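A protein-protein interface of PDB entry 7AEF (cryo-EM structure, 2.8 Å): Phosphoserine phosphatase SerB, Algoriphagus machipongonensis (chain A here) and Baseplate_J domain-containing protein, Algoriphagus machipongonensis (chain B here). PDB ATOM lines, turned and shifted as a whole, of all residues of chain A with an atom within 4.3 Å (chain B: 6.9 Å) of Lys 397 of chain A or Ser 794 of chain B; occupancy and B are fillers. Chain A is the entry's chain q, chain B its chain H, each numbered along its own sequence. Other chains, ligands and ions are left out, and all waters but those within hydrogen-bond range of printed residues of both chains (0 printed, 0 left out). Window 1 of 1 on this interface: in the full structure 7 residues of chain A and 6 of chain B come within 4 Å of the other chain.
O of Glu 404 of chain A sits at hydrogen-bond distance from N of Ser 794 of chain B (3.0 Å). The side-chain carboxylate (OE1) of Glu 405 of chain A is in hydrogen-bond range of the backbone NH (N) of Arg 792 of chain B (3.4 Å).
The backbone carbonyl oxygen (O) of Leu 381 of chain A lies within hydrogen-bond range of the backbone NH (N) of Lys 397 of chain A (2.8 Å). The side-chain hydroxyl (OG1) of Thr 383 of chain A is in hydrogen-bond range of the backbone carbonyl oxygen (O) of Glu 406 of chain A (2.8 Å). NZ of Lys 397 of chain A lies within hydrogen-bond range of O of Asn 403 of chain A.
Among the printed residues, merely in contact across the chains: Glu 404 of chain A with Leu 793 of chain B, Glu 405 of chain A with Ser 794 of chain B, Glu 406 of chain A with Arg 792 of chain B, Lys 397 of chain A with Ser 794 of chain B, Glu 405 of chain A with Glu 791 of chain B, Glu 404 of chain A with Arg 792 of chain B and Glu 406 of chain A with Leu 793 of chain B.
Of the printed residues of chain B, Glu 405 of chain A touches Glu 791 (3.96 Å), Arg 792 (3.1 Å) and Ser 794 (3.8 Å). Of the printed residues of chain B, Glu 406 of chain A touches Arg 792 and Leu 793. Val 170 of chain B touches none of the printed residues of chain A. Of the printed residues of chain A, Arg 792 of chain B touches Glu 404, Glu 405 and Glu 406. Of the printed residues of chain A, Leu 793 of chain B touches Glu 404 and Glu 406. Of the printed residues of chain A, Ser 794 of chain B touches Lys 397, Glu 404 and Glu 405. The nearest printed residue of chain B that does not touch Lys 397 of chain A is Trp 795 of chain B (6.9 Å). The nearest residue of chain A that does not touch Ser 794 of chain B is Thr 383 of chain A (4.02 Å). The nearest printed residue of chain B that does not touch Glu 405 of chain A is Leu 793 of chain B (4.7 Å).
Printed residues of chain B that touch a printed residue of chain A: Glu 791, Arg 792, Leu 793 and Ser 794. Along chain B the printed residues that touch a printed residue of chain A span positions 791 to 794. Among the printed residues, 9 pairs touch across the chains.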
ATOM      1  N   GLY A 380      23.073  16.945  -6.651  1.00  0.00           N
ATOM      2  CA  GLY A 380      21.731  16.946  -7.237  1.00  0.00           C
ATOM      3  C   GLY A 380      21.593  17.721  -8.557  1.00  0.00           C
ATOM      4  O   GLY A 380      22.504  18.427  -8.989  1.00  0.00           O
ATOM      5  N   LEU A 381      20.394  17.644  -9.150  1.00  0.00           N
ATOM      6  CA  LEU A 381      20.058  18.327 -10.414  1.00  0.00           C
ATOM      7  C   LEU A 381      18.879  19.276 -10.278  1.00  0.00           C
ATOM      8  O   LEU A 381      17.877  18.955  -9.646  1.00  0.00           O
ATOM      9  CB  LEU A 381      19.740  17.294 -11.494  1.00  0.00           C
ATOM     10  CG  LEU A 381      20.868  16.316 -11.866  1.00  0.00           C
ATOM     11  CD1 LEU A 381      20.321  15.263 -12.768  1.00  0.00           C
ATOM     12  CD2 LEU A 381      21.993  17.058 -12.565  1.00  0.00           C
ATOM     13  N   THR A 383      15.482  21.133 -11.242  1.00  0.00           N
ATOM     14  CA  THR A 383      14.296  20.894 -12.068  1.00  0.00           C
ATOM     15  C   THR A 383      13.272  22.042 -12.118  1.00  0.00           C
ATOM     16  O   THR A 383      12.501  22.109 -13.076  1.00  0.00           O
ATOM     17  CB  THR A 383      13.564  19.601 -11.618  1.00  0.00           C
ATOM     18  OG1 THR A 383      13.116  19.729 -10.264  1.00  0.00           O
ATOM     19  CG2 THR A 383      14.488  18.462 -11.698  1.00  0.00           C
ATOM     20  N   VAL A 396      15.183  20.576  -6.549  1.00  0.00           N
ATOM     21  CA  VAL A 396      16.333  19.726  -6.884  1.00  0.00           C
ATOM     22  C   VAL A 396      16.147  18.198  -6.687  1.00  0.00           C
ATOM     23  O   VAL A 396      15.650  17.747  -5.650  1.00  0.00           O
ATOM     24  CB  VAL A 396      17.547  20.184  -6.014  1.00  0.00           C
ATOM     25  CG1 VAL A 396      18.781  19.348  -6.260  1.00  0.00           C
ATOM     26  CG2 VAL A 396      17.866  21.631  -6.301  1.00  0.00           C
ATOM     27  N   LYS A 397      16.543  17.401  -7.694  1.00  0.00           N
ATOM     28  CA  LYS A 397      16.517  15.935  -7.600  1.00  0.00           C
ATOM     29  C   LYS A 397      17.804  15.466  -6.997  1.00  0.00           C
ATOM     30  O   LYS A 397      18.868  15.970  -7.354  1.00  0.00           O
ATOM     31  CB  LYS A 397      16.481  15.211  -8.940  1.00  0.00           C
ATOM     32  CG  LYS A 397      15.348  15.465  -9.768  1.00  0.00           C
ATOM     33  CD  LYS A 397      15.208  14.448 -10.929  1.00  0.00           C
ATOM     34  CE  LYS A 397      16.309  14.503 -11.946  1.00  0.00           C
ATOM     35  NZ  LYS A 397      15.994  13.638 -13.131  1.00  0.00           N
ATOM     36  N   ILE A 398      17.752  14.429  -6.190  1.00  0.00           N
ATOM     37  CA  ILE A 398      18.972  13.835  -5.700  1.00  0.00           C
ATOM     38  C   ILE A 398      19.030  12.390  -6.213  1.00  0.00           C
ATOM     39  O   ILE A 398      18.362  11.539  -5.628  1.00  0.00           O
ATOM     40  CB  ILE A 398      19.024  13.913  -4.174  1.00  0.00           C
ATOM     41  CG1 ILE A 398      18.950  15.409  -3.749  1.00  0.00           C
ATOM     42  CG2 ILE A 398      20.290  13.247  -3.678  1.00  0.00           C
ATOM     43  CD1 ILE A 398      18.801  15.657  -2.286  1.00  0.00           C
ATOM     44  N   PRO A 399      19.866  12.076  -7.225  1.00  0.00           N
ATOM     45  CA  PRO A 399      19.989  10.811  -7.928  1.00  0.00           C
ATOM     46  C   PRO A 399      20.303   9.592  -7.088  1.00  0.00           C
ATOM     47  O   PRO A 399      20.014   8.478  -7.506  1.00  0.00           O
ATOM     48  CB  PRO A 399      21.153  11.081  -8.870  1.00  0.00           C
ATOM     49  CG  PRO A 399      21.145  12.540  -9.074  1.00  0.00           C
ATOM     50  CD  PRO A 399      20.716  13.107  -7.802  1.00  0.00           C
ATOM     51  N   ASN A 403      16.297   9.264  -9.237  1.00  0.00           N
ATOM     52  CA  ASN A 403      16.670  10.123 -10.355  1.00  0.00           C
ATOM     53  C   ASN A 403      15.558  10.329 -11.402  1.00  0.00           C
ATOM     54  O   ASN A 403      15.841  10.784 -12.515  1.00  0.00           O
ATOM     55  CB  ASN A 403      17.919   9.563 -11.012  1.00  0.00           C
ATOM     56  CG  ASN A 403      18.685  10.584 -11.788  1.00  0.00           C
ATOM     57  OD1 ASN A 403      18.723  11.756 -11.402  1.00  0.00           O
ATOM     58  ND2 ASN A 403      19.310  10.171 -12.854  1.00  0.00           N
ATOM     59  N   GLU A 404      14.313   9.986 -11.068  1.00  0.00           N
ATOM     60  CA  GLU A 404      13.192  10.099 -12.007  1.00  0.00           C
ATOM     61  C   GLU A 404      12.112  11.112 -11.619  1.00  0.00           C
ATOM     62  O   GLU A 404      11.491  11.714 -12.494  1.00  0.00           O
ATOM     63  CB  GLU A 404      12.535   8.739 -12.186  1.00  0.00           C
ATOM     64  CG  GLU A 404      13.433   7.690 -12.796  1.00  0.00           C
ATOM     65  CD  GLU A 404      12.751   6.367 -12.969  1.00  0.00           C
ATOM     66  OE1 GLU A 404      11.618   6.254 -12.568  1.00  0.00           O
ATOM     67  OE2 GLU A 404      13.359   5.467 -13.501  1.00  0.00           O
ATOM     68  N   GLU A 405      11.843  11.306 -10.346  1.00  0.00           N
ATOM     69  CA  GLU A 405      10.800  12.220  -9.969  1.00  0.00           C
ATOM     70  C   GLU A 405      11.225  13.636  -9.922  1.00  0.00           C
ATOM     71  O   GLU A 405      12.339  13.944 -10.242  1.00  0.00           O
ATOM     72  CB  GLU A 405      10.108  11.741  -8.734  1.00  0.00           C
ATOM     73  CG  GLU A 405       9.578  10.358  -8.998  1.00  0.00           C
ATOM     74  CD  GLU A 405       8.681   9.869  -7.913  1.00  0.00           C
ATOM     75  OE1 GLU A 405       7.564  10.388  -7.805  1.00  0.00           O
ATOM     76  OE2 GLU A 405       9.085   8.955  -7.170  1.00  0.00           O
ATOM     77  N   GLU A 406      10.322  14.508  -9.535  1.00  0.00           N
ATOM     78  CA  GLU A 406      10.578  15.949  -9.542  1.00  0.00           C
ATOM     79  C   GLU A 406      11.635  16.497  -8.570  1.00  0.00           C
ATOM     80  O   GLU A 406      12.322  17.471  -8.902  1.00  0.00           O
ATOM     81  CB  GLU A 406       9.277  16.675  -9.271  1.00  0.00           C
ATOM     82  CG  GLU A 406       8.262  16.592 -10.365  1.00  0.00           C
ATOM     83  CD  GLU A 406       6.996  17.276  -9.981  1.00  0.00           C
ATOM     84  OE1 GLU A 406       6.794  17.463  -8.801  1.00  0.00           O
ATOM     85  OE2 GLU A 406       6.236  17.623 -10.845  1.00  0.00           O
ATOM     86  N   GLY A 407      11.734  15.923  -7.364  1.00  0.00           N
ATOM     87  CA  GLY A 407      12.668  16.423  -6.343  1.00  0.00           C
ATOM     88  C   GLY A 407      12.014  17.263  -5.239  1.00  0.00           C
ATOM     89  O   GLY A 407      10.792  17.260  -5.082  1.00  0.00           O
ATOM     90  N   ALA B 167       8.333  19.782 -20.174  1.00  0.00           N
ATOM     91  CA  ALA B 167       9.237  20.648 -19.422  1.00  0.00           C
ATOM     92  C   ALA B 167      10.220  21.347 -20.355  1.00  0.00           C
ATOM     93  O   ALA B 167      10.331  20.996 -21.504  1.00  0.00           O
ATOM     94  CB  ALA B 167       9.962  19.860 -18.354  1.00  0.00           C
ATOM     95  N   ASN B 169      13.662  21.578 -20.957  1.00  0.00           N
ATOM     96  CA  ASN B 169      14.811  21.006 -21.651  1.00  0.00           C
ATOM     97  C   ASN B 169      14.567  19.784 -22.549  1.00  0.00           C
ATOM     98  O   ASN B 169      15.540  19.202 -23.019  1.00  0.00           O
ATOM     99  CB  ASN B 169      15.842  20.623 -20.607  1.00  0.00           C
ATOM    100  CG  ASN B 169      15.220  19.944 -19.414  1.00  0.00           C
ATOM    101  OD1 ASN B 169      14.444  20.543 -18.704  1.00  0.00           O
ATOM    102  ND2 ASN B 169      15.538  18.683 -19.208  1.00  0.00           N
ATOM    103  N   VAL B 170      13.325  19.387 -22.813  1.00  0.00           N
ATOM    104  CA  VAL B 170      13.061  18.192 -23.627  1.00  0.00           C
ATOM    105  C   VAL B 170      12.306  18.510 -24.917  1.00  0.00           C
ATOM    106  O   VAL B 170      11.486  19.425 -24.949  1.00  0.00           O
ATOM    107  CB  VAL B 170      12.274  17.133 -22.829  1.00  0.00           C
ATOM    108  CG1 VAL B 170      13.080  16.667 -21.629  1.00  0.00           C
ATOM    109  CG2 VAL B 170      10.927  17.684 -22.390  1.00  0.00           C
ATOM    110  N   GLU B 791       3.462   8.543 -10.518  1.00  0.00           N
ATOM    111  CA  GLU B 791       4.836   8.844 -10.217  1.00  0.00           C
ATOM    112  C   GLU B 791       5.022  10.127 -10.945  1.00  0.00           C
ATOM    113  O   GLU B 791       4.928  10.155 -12.146  1.00  0.00           O
ATOM    114  CB  GLU B 791       5.815   7.882 -10.841  1.00  0.00           C
ATOM    115  CG  GLU B 791       5.314   6.491 -11.086  1.00  0.00           C
ATOM    116  CD  GLU B 791       6.269   5.714 -11.970  1.00  0.00           C
ATOM    117  OE1 GLU B 791       7.346   6.253 -12.281  1.00  0.00           O
ATOM    118  OE2 GLU B 791       5.943   4.572 -12.360  1.00  0.00           O
ATOM    119  N   ARG B 792       5.323  11.192 -10.243  1.00  0.00           N
ATOM    120  CA  ARG B 792       5.526  12.441 -10.909  1.00  0.00           C
ATOM    121  C   ARG B 792       6.855  12.307 -11.618  1.00  0.00           C
ATOM    122  O   ARG B 792       7.811  11.964 -11.023  1.00  0.00           O
ATOM    123  CB  ARG B 792       5.540  13.520  -9.847  1.00  0.00           C
ATOM    124  CG  ARG B 792       4.425  13.324  -8.841  1.00  0.00           C
ATOM    125  CD  ARG B 792       4.069  14.605  -8.134  1.00  0.00           C
ATOM    126  NE  ARG B 792       2.865  14.454  -7.334  1.00  0.00           N
ATOM    127  CZ  ARG B 792       2.351  15.421  -6.595  1.00  0.00           C
ATOM    128  NH1 ARG B 792       2.932  16.592  -6.561  1.00  0.00           N
ATOM    129  NH2 ARG B 792       1.261  15.222  -5.899  1.00  0.00           N
ATOM    130  N   LEU B 793       6.842  12.416 -12.932  1.00  0.00           N
ATOM    131  CA  LEU B 793       8.028  12.322 -13.745  1.00  0.00           C
ATOM    132  C   LEU B 793       8.578  13.705 -13.891  1.00  0.00           C
ATOM    133  O   LEU B 793       7.857  14.680 -13.848  1.00  0.00           O
ATOM    134  CB  LEU B 793       7.707  11.748 -15.108  1.00  0.00           C
ATOM    135  CG  LEU B 793       7.220  10.311 -15.165  1.00  0.00           C
ATOM    136  CD1 LEU B 793       7.000   9.954 -16.607  1.00  0.00           C
ATOM    137  CD2 LEU B 793       8.219   9.354 -14.559  1.00  0.00           C
ATOM    138  N   SER B 794       9.878  13.775 -14.029  1.00  0.00           N
ATOM    139  CA  SER B 794      10.600  15.011 -14.164  1.00  0.00           C
ATOM    140  C   SER B 794      10.331  15.860 -15.425  1.00  0.00           C
ATOM    141  O   SER B 794      10.231  17.059 -15.328  1.00  0.00           O
ATOM    142  CB  SER B 794      12.065  14.670 -14.009  1.00  0.00           C
ATOM    143  OG  SER B 794      12.873  15.768 -14.210  1.00  0.00           O
ATOM    144  N   TRP B 795      10.191  15.235 -16.588  1.00  0.00           N
ATOM    145  CA  TRP B 795       9.980  15.924 -17.855  1.00  0.00           C
ATOM    146  C   TRP B 795       8.599  16.479 -18.156  1.00  0.00           C
ATOM    147  O   TRP B 795       8.418  17.179 -19.119  1.00  0.00           O
ATOM    148  CB  TRP B 795      10.467  15.082 -19.022  1.00  0.00           C
ATOM    149  CG  TRP B 795      10.000  13.693 -19.029  1.00  0.00           C
ATOM    150  CD1 TRP B 795      10.545  12.663 -18.364  1.00  0.00           C
ATOM    151  CD2 TRP B 795       8.900  13.161 -19.764  1.00  0.00           C
ATOM    152  NE1 TRP B 795       9.854  11.518 -18.619  1.00  0.00           N
ATOM    153  CE2 TRP B 795       8.832  11.804 -19.475  1.00  0.00           C
ATOM    154  CE3 TRP B 795       7.955  13.711 -20.632  1.00  0.00           C
ATOM    155  CZ2 TRP B 795       7.870  10.975 -20.030  1.00  0.00           C
ATOM    156  CZ3 TRP B 795       7.004  12.892 -21.172  1.00  0.00           C
ATOM    157  CH2 TRP B 795       6.960  11.542 -20.870  1.00  0.00           C
ATOM    158  N   ILE B 796       7.619  16.154 -17.349  1.00  0.00           N
ATOM    159  CA  ILE B 796       6.309  16.666 -17.574  1.00  0.00           C
ATOM    160  C   ILE B 796       6.047  17.904 -16.779  1.00  0.00           C
ATOM    161  O   ILE B 796       5.875  17.827 -15.606  1.00  0.00           O
ATOM    162  CB  ILE B 796       5.268  15.658 -17.068  1.00  0.00           C
ATOM    163  CG1 ILE B 796       5.268  14.406 -17.922  1.00  0.00           C
ATOM    164  CG2 ILE B 796       3.880  16.274 -17.011  1.00  0.00           C
ATOM    165  CD1 ILE B 796       4.866  13.193 -17.142  1.00  0.00           C
ATOM    166  N   LYS B 797       5.981  19.046 -17.434  1.00  0.00           N
ATOM    167  CA  LYS B 797       5.614  20.257 -16.747  1.00  0.00           C
ATOM    168  C   LYS B 797       4.169  20.168 -16.426  1.00  0.00           C
ATOM    169  O   LYS B 797       3.787  20.578 -15.344  1.00  0.00           O
ATOM    170  CB  LYS B 797       5.863  21.517 -17.545  1.00  0.00           C
ATOM    171  CG  LYS B 797       5.729  22.767 -16.714  1.00  0.00           C
ATOM    172  CD  LYS B 797       5.906  24.006 -17.553  1.00  0.00           C
ATOM    173  CE  LYS B 797       5.910  25.243 -16.674  1.00  0.00           C
ATOM    174  NZ  LYS B 797       6.754  26.362 -17.192  1.00  0.00           N
